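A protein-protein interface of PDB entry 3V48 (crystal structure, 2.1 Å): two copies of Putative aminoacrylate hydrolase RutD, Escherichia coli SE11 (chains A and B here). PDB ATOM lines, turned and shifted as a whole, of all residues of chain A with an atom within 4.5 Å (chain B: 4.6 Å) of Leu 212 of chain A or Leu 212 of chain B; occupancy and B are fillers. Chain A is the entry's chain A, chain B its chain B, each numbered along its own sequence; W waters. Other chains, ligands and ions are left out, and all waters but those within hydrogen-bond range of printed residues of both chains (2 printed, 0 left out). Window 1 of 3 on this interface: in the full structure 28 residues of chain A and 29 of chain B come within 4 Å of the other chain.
CE1 of His 122 of chain A touches CD2 of Leu 148 of chain B, at 3.5 Å. CB of Ala 153 of chain B touches NE2 of His 122 of chain A (3.6 Å). CE1 of His 122 of chain B touches CD2 of Leu 148 of chain A, 3.5 Å away. Leu 212 of chain B touches Leu 148 of chain A (CD1 to O, 3.5 Å). NE2 of His 122 of chain B touches CB of Ala 153 of chain A, at 3.6 Å. Ala 153 of chain A touches Asp 211 of chain B (CB to O, 3.1 Å). Ala 153 of chain A touches Leu 212 of chain B (CB to O, 3.6 Å). Leu 148 of chain B touches Leu 212 of chain A. CB of Ala 153 of chain B touches O of Leu 212 of chain A, 3.6 Å away. CD2 of Leu 212 of chain A touches CD2 of Leu 212 of chain B, 3.2 Å away.
Water W1 lies within hydrogen-bond range of the backbone carbonyl oxygen of Asp 211 of chain B (2.9 Å) and the backbone NH of Ala 153 of chain A (2.9 Å). Water W2 bridges the backbone carbonyl oxygen (O) of Asp 211 of chain A and the backbone NH (N) of Ala 153 of chain B.
His 122 of chain A touches Ala 153 of chain B, and with the chains exchanged Ala 153 of chain A touches His 122 of chain B. Cys 126 of chain A touches Leu 148 of chain B, and with the chains exchanged Leu 148 of chain A touches Cys 126 of chain B. Leu 148 of chain A touches Leu 212 of chain B, and with the chains exchanged Leu 212 of chain A touches Leu 148 of chain B. Ala 153 of chain A touches Leu 212 of chain B, and with the chains exchanged Leu 212 of chain A touches Ala 153 of chain B.
The backbone carbonyl oxygen of His 122 of chain A sits at hydrogen-bond distance from the side-chain sulfur of Cys 126 of chain A (3.5 Å). O of Leu 212 of chain A lies within hydrogen-bond range of NE2 of His 122 of chain A (2.6 Å). The side-chain sulfur of Cys 126 of chain A is in hydrogen-bond range of the backbone carbonyl oxygen of Leu 212 of chain A (3.8 Å). The backbone carbonyl oxygen of His 122 of chain B sits at hydrogen-bond distance from the side-chain sulfur of Cys 126 of chain B, at 3.5 Å. SG of Cys 126 of chain B is in hydrogen-bond range of O of Leu 212 of chain B, at 3.8 Å. The side-chain carboxylate of Asp 211 of chain B sits at hydrogen-bond distance from the backbone NH of Leu 213 of chain B, 2.8 Å away.
Leu 212 of chain A touches just these residues of chain B: Leu 148 (3.5 Å), Ala 153 (3.6 Å) and Leu 212 (3.2 Å). Leu 212 of chain B touches three residues of chain A. Of the printed residues of chain B, Asp 211 of chain A touches Ala 153. Of the printed residues of chain A, Leu 148 of chain B touches His 122, Cys 126 and Leu 212.
Along chain A the printed residues that touch a printed residue of chain B span positions 122 to 212. Hydrophobic or aromatic side chains of chain B that line the printed part of chain A: His 122, Leu 148, Ala 153 and Leu 212. Among the printed residues, no Asp or Glu carboxylate lies within 4 Å of a Lys or Arg side-chain nitrogen of the other chain.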
ATOM      1  N   HIS A 122     -25.527 -12.258  -7.940  1.00  0.00           N
ATOM      2  CA  HIS A 122     -26.022 -13.511  -8.531  1.00  0.00           C
ATOM      3  C   HIS A 122     -26.613 -14.465  -7.505  1.00  0.00           C
ATOM      4  O   HIS A 122     -27.708 -14.988  -7.666  1.00  0.00           O
ATOM      5  CB  HIS A 122     -24.928 -14.234  -9.283  1.00  0.00           C
ATOM      6  CG  HIS A 122     -25.401 -15.516  -9.918  1.00  0.00           C
ATOM      7  ND1 HIS A 122     -25.980 -15.548 -11.122  1.00  0.00           N
ATOM      8  CD2 HIS A 122     -25.391 -16.816  -9.452  1.00  0.00           C
ATOM      9  CE1 HIS A 122     -26.317 -16.799 -11.420  1.00  0.00           C
ATOM     10  NE2 HIS A 122     -25.956 -17.578 -10.394  1.00  0.00           N
ATOM     11  N   CYS A 126     -30.422 -15.820  -6.978  1.00  0.00           N
ATOM     12  CA  CYS A 126     -30.794 -17.218  -6.731  1.00  0.00           C
ATOM     13  C   CYS A 126     -31.664 -17.364  -5.476  1.00  0.00           C
ATOM     14  O   CYS A 126     -32.716 -18.012  -5.500  1.00  0.00           O
ATOM     15  CB  CYS A 126     -29.540 -18.108  -6.585  1.00  0.00           C
ATOM     16  SG  CYS A 126     -28.617 -18.306  -8.158  1.00  0.00           S
ATOM     17  N   LEU A 148     -31.456 -28.201  -8.336  1.00  0.00           N
ATOM     18  CA  LEU A 148     -31.091 -27.397  -9.500  1.00  0.00           C
ATOM     19  C   LEU A 148     -29.938 -26.418  -9.210  1.00  0.00           C
ATOM     20  O   LEU A 148     -29.203 -26.029 -10.121  1.00  0.00           O
ATOM     21  CB  LEU A 148     -32.280 -26.650 -10.047  1.00  0.00           C
ATOM     22  CG  LEU A 148     -33.498 -27.516 -10.392  1.00  0.00           C
ATOM     23  CD1 LEU A 148     -34.719 -26.643 -10.642  1.00  0.00           C
ATOM     24  CD2 LEU A 148     -33.091 -28.362 -11.609  1.00  0.00           C
ATOM     25  N   PHE A 149     -29.823 -26.014  -7.945  1.00  0.00           N
ATOM     26  CA  PHE A 149     -28.805 -25.093  -7.516  1.00  0.00           C
ATOM     27  C   PHE A 149     -27.545 -25.780  -7.039  1.00  0.00           C
ATOM     28  O   PHE A 149     -26.507 -25.130  -6.896  1.00  0.00           O
ATOM     29  CB  PHE A 149     -29.354 -24.174  -6.417  1.00  0.00           C
ATOM     30  CG  PHE A 149     -30.409 -23.272  -6.924  1.00  0.00           C
ATOM     31  CD1 PHE A 149     -30.060 -22.093  -7.519  1.00  0.00           C
ATOM     32  CD2 PHE A 149     -31.748 -23.654  -6.885  1.00  0.00           C
ATOM     33  CE1 PHE A 149     -31.024 -21.277  -8.059  1.00  0.00           C
ATOM     34  CE2 PHE A 149     -32.733 -22.842  -7.410  1.00  0.00           C
ATOM     35  CZ  PHE A 149     -32.372 -21.659  -8.020  1.00  0.00           C
ATOM     36  N   TYR A 151     -26.440 -29.354  -8.250  1.00  0.00           N
ATOM     37  CA  TYR A 151     -25.863 -30.385  -9.084  1.00  0.00           C
ATOM     38  C   TYR A 151     -25.920 -30.057 -10.576  1.00  0.00           C
ATOM     39  O   TYR A 151     -26.857 -29.397 -11.034  1.00  0.00           O
ATOM     40  CB  TYR A 151     -26.643 -31.668  -8.898  1.00  0.00           C
ATOM     41  CG  TYR A 151     -26.848 -32.133  -7.497  1.00  0.00           C
ATOM     42  CD1 TYR A 151     -25.803 -32.213  -6.605  1.00  0.00           C
ATOM     43  CD2 TYR A 151     -28.077 -32.604  -7.098  1.00  0.00           C
ATOM     44  CE1 TYR A 151     -25.974 -32.714  -5.345  1.00  0.00           C
ATOM     45  CE2 TYR A 151     -28.268 -33.107  -5.831  1.00  0.00           C
ATOM     46  CZ  TYR A 151     -27.208 -33.145  -4.964  1.00  0.00           C
ATOM     47  OH  TYR A 151     -27.381 -33.651  -3.713  1.00  0.00           O
ATOM     48  N   ALA A 153     -26.931 -30.757 -14.352  1.00  0.00           N
ATOM     49  CA  ALA A 153     -28.098 -31.377 -14.962  1.00  0.00           C
ATOM     50  C   ALA A 153     -27.866 -32.853 -15.301  1.00  0.00           C
ATOM     51  O   ALA A 153     -28.680 -33.679 -14.974  1.00  0.00           O
ATOM     52  CB  ALA A 153     -28.572 -30.583 -16.204  1.00  0.00           C
ATOM     53  N   ASP A 210     -18.818 -24.804 -12.761  1.00  0.00           N
ATOM     54  CA  ASP A 210     -20.211 -24.913 -13.068  1.00  0.00           C
ATOM     55  C   ASP A 210     -21.130 -24.698 -11.866  1.00  0.00           C
ATOM     56  O   ASP A 210     -22.303 -25.046 -11.939  1.00  0.00           O
ATOM     57  CB  ASP A 210     -20.529 -26.242 -13.742  1.00  0.00           C
ATOM     58  CG  ASP A 210     -20.189 -27.440 -12.877  1.00  0.00           C
ATOM     59  OD1 ASP A 210     -19.540 -27.243 -11.813  1.00  0.00           O
ATOM     60  OD2 ASP A 210     -20.505 -28.585 -13.308  1.00  0.00           O
ATOM     61  N   ASP A 211     -20.620 -24.114 -10.791  1.00  0.00           N
ATOM     62  CA  ASP A 211     -21.448 -23.787  -9.638  1.00  0.00           C
ATOM     63  C   ASP A 211     -22.513 -22.765 -10.080  1.00  0.00           C
ATOM     64  O   ASP A 211     -22.164 -21.721 -10.586  1.00  0.00           O
ATOM     65  CB  ASP A 211     -20.592 -23.198  -8.538  1.00  0.00           C
ATOM     66  CG  ASP A 211     -21.375 -22.942  -7.264  1.00  0.00           C
ATOM     67  OD1 ASP A 211     -22.613 -22.768  -7.352  1.00  0.00           O
ATOM     68  OD2 ASP A 211     -20.764 -23.002  -6.184  1.00  0.00           O
ATOM     69  N   LEU A 212     -23.792 -23.119  -9.960  1.00  0.00           N
ATOM     70  CA  LEU A 212     -24.887 -22.244 -10.395  1.00  0.00           C
ATOM     71  C   LEU A 212     -25.231 -21.201  -9.320  1.00  0.00           C
ATOM     72  O   LEU A 212     -25.662 -20.100  -9.656  1.00  0.00           O
ATOM     73  CB  LEU A 212     -26.155 -23.041 -10.743  1.00  0.00           C
ATOM     74  CG  LEU A 212     -27.206 -22.176 -11.450  1.00  0.00           C
ATOM     75  CD1 LEU A 212     -26.775 -21.975 -12.892  1.00  0.00           C
ATOM     76  CD2 LEU A 212     -28.657 -22.664 -11.324  1.00  0.00           C
ATOM     77  N   LEU A 213     -25.038 -21.552  -8.036  1.00  0.00           N
ATOM     78  CA  LEU A 213     -25.504 -20.726  -6.954  1.00  0.00           C
ATOM     79  C   LEU A 213     -24.512 -19.608  -6.580  1.00  0.00           C
ATOM     80  O   LEU A 213     -24.899 -18.477  -6.290  1.00  0.00           O
ATOM     81  CB  LEU A 213     -25.840 -21.599  -5.743  1.00  0.00           C
ATOM     82  CG  LEU A 213     -26.379 -20.902  -4.481  1.00  0.00           C
ATOM     83  CD1 LEU A 213     -27.717 -20.238  -4.778  1.00  0.00           C
ATOM     84  CD2 LEU A 213     -26.480 -21.897  -3.344  1.00  0.00           C
ATOM     85  N   VAL A 214     -23.237 -19.950  -6.596  1.00  0.00           N
ATOM     86  CA  VAL A 214     -22.128 -19.048  -6.286  1.00  0.00           C
ATOM     87  C   VAL A 214     -21.163 -19.028  -7.478  1.00  0.00           C
ATOM     88  O   VAL A 214     -20.534 -20.028  -7.762  1.00  0.00           O
ATOM     89  CB  VAL A 214     -21.346 -19.509  -5.025  1.00  0.00           C
ATOM     90  CG1 VAL A 214     -20.231 -18.524  -4.695  1.00  0.00           C
ATOM     91  CG2 VAL A 214     -22.294 -19.607  -3.847  1.00  0.00           C
ATOM     92  N   HIS B 122     -35.865 -34.278 -15.869  1.00  0.00           N
ATOM     93  CA  HIS B 122     -35.130 -33.126 -15.367  1.00  0.00           C
ATOM     94  C   HIS B 122     -35.703 -31.784 -15.869  1.00  0.00           C
ATOM     95  O   HIS B 122     -35.928 -30.853 -15.119  1.00  0.00           O
ATOM     96  CB  HIS B 122     -33.649 -33.212 -15.721  1.00  0.00           C
ATOM     97  CG  HIS B 122     -32.871 -32.023 -15.231  1.00  0.00           C
ATOM     98  ND1 HIS B 122     -32.368 -31.944 -13.964  1.00  0.00           N
ATOM     99  CD2 HIS B 122     -32.590 -30.808 -15.833  1.00  0.00           C
ATOM    100  CE1 HIS B 122     -31.762 -30.761 -13.801  1.00  0.00           C
ATOM    101  NE2 HIS B 122     -31.910 -30.059 -14.932  1.00  0.00           N
ATOM    102  N   CYS B 126     -37.518 -28.683 -13.942  1.00  0.00           N
ATOM    103  CA  CYS B 126     -37.189 -27.282 -14.146  1.00  0.00           C
ATOM    104  C   CYS B 126     -38.477 -26.489 -14.423  1.00  0.00           C
ATOM    105  O   CYS B 126     -38.708 -25.449 -13.809  1.00  0.00           O
ATOM    106  CB  CYS B 126     -36.174 -27.098 -15.278  1.00  0.00           C
ATOM    107  SG  CYS B 126     -34.520 -27.705 -14.909  1.00  0.00           S
ATOM    108  N   LEU B 148     -31.156 -17.953 -14.957  1.00  0.00           N
ATOM    109  CA  LEU B 148     -30.486 -19.007 -14.147  1.00  0.00           C
ATOM    110  C   LEU B 148     -30.541 -20.359 -14.866  1.00  0.00           C
ATOM    111  O   LEU B 148     -29.737 -21.212 -14.620  1.00  0.00           O
ATOM    112  CB  LEU B 148     -31.125 -19.155 -12.771  1.00  0.00           C
ATOM    113  CG  LEU B 148     -31.158 -17.867 -11.928  1.00  0.00           C
ATOM    114  CD1 LEU B 148     -31.975 -18.149 -10.674  1.00  0.00           C
ATOM    115  CD2 LEU B 148     -29.752 -17.372 -11.634  1.00  0.00           C
ATOM    116  N   PHE B 149     -31.505 -20.527 -15.752  1.00  0.00           N
ATOM    117  CA  PHE B 149     -31.648 -21.731 -16.587  1.00  0.00           C
ATOM    118  C   PHE B 149     -30.911 -21.670 -17.926  1.00  0.00           C
ATOM    119  O   PHE B 149     -30.786 -22.700 -18.580  1.00  0.00           O
ATOM    120  CB  PHE B 149     -33.149 -22.022 -16.792  1.00  0.00           C
ATOM    121  CG  PHE B 149     -33.830 -22.414 -15.520  1.00  0.00           C
ATOM    122  CD1 PHE B 149     -33.798 -23.712 -15.082  1.00  0.00           C
ATOM    123  CD2 PHE B 149     -34.399 -21.448 -14.710  1.00  0.00           C
ATOM    124  CE1 PHE B 149     -34.396 -24.080 -13.875  1.00  0.00           C
ATOM    125  CE2 PHE B 149     -34.979 -21.783 -13.511  1.00  0.00           C
ATOM    126  CZ  PHE B 149     -34.983 -23.105 -13.085  1.00  0.00           C
ATOM    127  N   TYR B 151     -27.857 -19.301 -18.617  1.00  0.00           N
ATOM    128  CA  TYR B 151     -26.473 -18.851 -18.647  1.00  0.00           C
ATOM    129  C   TYR B 151     -25.687 -19.458 -17.487  1.00  0.00           C
ATOM    130  O   TYR B 151     -26.231 -19.660 -16.412  1.00  0.00           O
ATOM    131  CB  TYR B 151     -26.401 -17.354 -18.522  1.00  0.00           C
ATOM    132  CG  TYR B 151     -27.202 -16.521 -19.490  1.00  0.00           C
ATOM    133  CD1 TYR B 151     -27.200 -16.781 -20.815  1.00  0.00           C
ATOM    134  CD2 TYR B 151     -27.869 -15.370 -19.048  1.00  0.00           C
ATOM    135  CE1 TYR B 151     -27.925 -16.012 -21.690  1.00  0.00           C
ATOM    136  CE2 TYR B 151     -28.568 -14.540 -19.923  1.00  0.00           C
ATOM    137  CZ  TYR B 151     -28.618 -14.889 -21.255  1.00  0.00           C
ATOM    138  OH  TYR B 151     -29.234 -14.089 -22.168  1.00  0.00           O
ATOM    139  N   ALA B 153     -23.425 -19.175 -14.225  1.00  0.00           N
ATOM    140  CA  ALA B 153     -23.333 -18.208 -13.141  1.00  0.00           C
ATOM    141  C   ALA B 153     -22.272 -17.140 -13.386  1.00  0.00           C
ATOM    142  O   ALA B 153     -22.540 -15.967 -13.235  1.00  0.00           O
ATOM    143  CB  ALA B 153     -23.008 -18.937 -11.840  1.00  0.00           C
ATOM    144  N   ASP B 210     -22.809 -27.916 -19.600  1.00  0.00           N
ATOM    145  CA  ASP B 210     -23.297 -27.235 -18.424  1.00  0.00           C
ATOM    146  C   ASP B 210     -24.711 -26.675 -18.594  1.00  0.00           C
ATOM    147  O   ASP B 210     -25.116 -25.826 -17.864  1.00  0.00           O
ATOM    148  CB  ASP B 210     -22.339 -26.130 -18.007  1.00  0.00           C
ATOM    149  CG  ASP B 210     -22.160 -25.062 -19.084  1.00  0.00           C
ATOM    150  OD1 ASP B 210     -22.598 -25.281 -20.254  1.00  0.00           O
ATOM    151  OD2 ASP B 210     -21.514 -24.016 -18.762  1.00  0.00           O
ATOM    152  N   ASP B 211     -25.441 -27.188 -19.562  1.00  0.00           N
ATOM    153  CA  ASP B 211     -26.832 -26.808 -19.767  1.00  0.00           C
ATOM    154  C   ASP B 211     -27.603 -27.281 -18.541  1.00  0.00           C
ATOM    155  O   ASP B 211     -27.594 -28.458 -18.241  1.00  0.00           O
ATOM    156  CB  ASP B 211     -27.386 -27.473 -21.031  1.00  0.00           C
ATOM    157  CG  ASP B 211     -28.800 -27.022 -21.359  1.00  0.00           C
ATOM    158  OD1 ASP B 211     -29.529 -26.615 -20.434  1.00  0.00           O
ATOM    159  OD2 ASP B 211     -29.168 -27.055 -22.544  1.00  0.00           O
ATOM    160  N   LEU B 212     -28.198 -26.339 -17.809  1.00  0.00           N
ATOM    161  CA  LEU B 212     -28.930 -26.655 -16.583  1.00  0.00           C
ATOM    162  C   LEU B 212     -30.359 -27.128 -16.885  1.00  0.00           C
ATOM    163  O   LEU B 212     -30.927 -27.894 -16.119  1.00  0.00           O
ATOM    164  CB  LEU B 212     -29.001 -25.423 -15.652  1.00  0.00           C
ATOM    165  CG  LEU B 212     -29.460 -25.790 -14.256  1.00  0.00           C
ATOM    166  CD1 LEU B 212     -28.357 -26.495 -13.480  1.00  0.00           C
ATOM    167  CD2 LEU B 212     -29.977 -24.546 -13.536  1.00  0.00           C
ATOM    168  N   LEU B 213     -30.933 -26.705 -18.006  1.00  0.00           N
ATOM    169  CA  LEU B 213     -32.360 -26.957 -18.272  1.00  0.00           C
ATOM    170  C   LEU B 213     -32.605 -28.287 -18.990  1.00  0.00           C
ATOM    171  O   LEU B 213     -33.569 -28.987 -18.705  1.00  0.00           O
ATOM    172  CB  LEU B 213     -32.958 -25.774 -19.072  1.00  0.00           C
ATOM    173  CG  LEU B 213     -34.456 -25.824 -19.409  1.00  0.00           C
ATOM    174  CD1 LEU B 213     -35.346 -25.996 -18.165  1.00  0.00           C
ATOM    175  CD2 LEU B 213     -34.842 -24.577 -20.209  1.00  0.00           C
ATOM    176  N   VAL B 214     -31.734 -28.582 -19.947  1.00  0.00           N
ATOM    177  CA  VAL B 214     -31.772 -29.795 -20.740  1.00  0.00           C
ATOM    178  C   VAL B 214     -30.444 -30.526 -20.557  1.00  0.00           C
ATOM    179  O   VAL B 214     -29.408 -30.039 -20.987  1.00  0.00           O
ATOM    180  CB  VAL B 214     -31.988 -29.451 -22.237  1.00  0.00           C
ATOM    181  CG1 VAL B 214     -32.168 -30.736 -23.056  1.00  0.00           C
ATOM    182  CG2 VAL B 214     -33.198 -28.526 -22.346  1.00  0.00           C
HETATM  183  O   HOH W   1     -25.686 -28.862 -16.130  1.00  0.00           O
HETATM  184  O   HOH W   2     -22.642 -21.896 -13.429  1.00  0.00           O
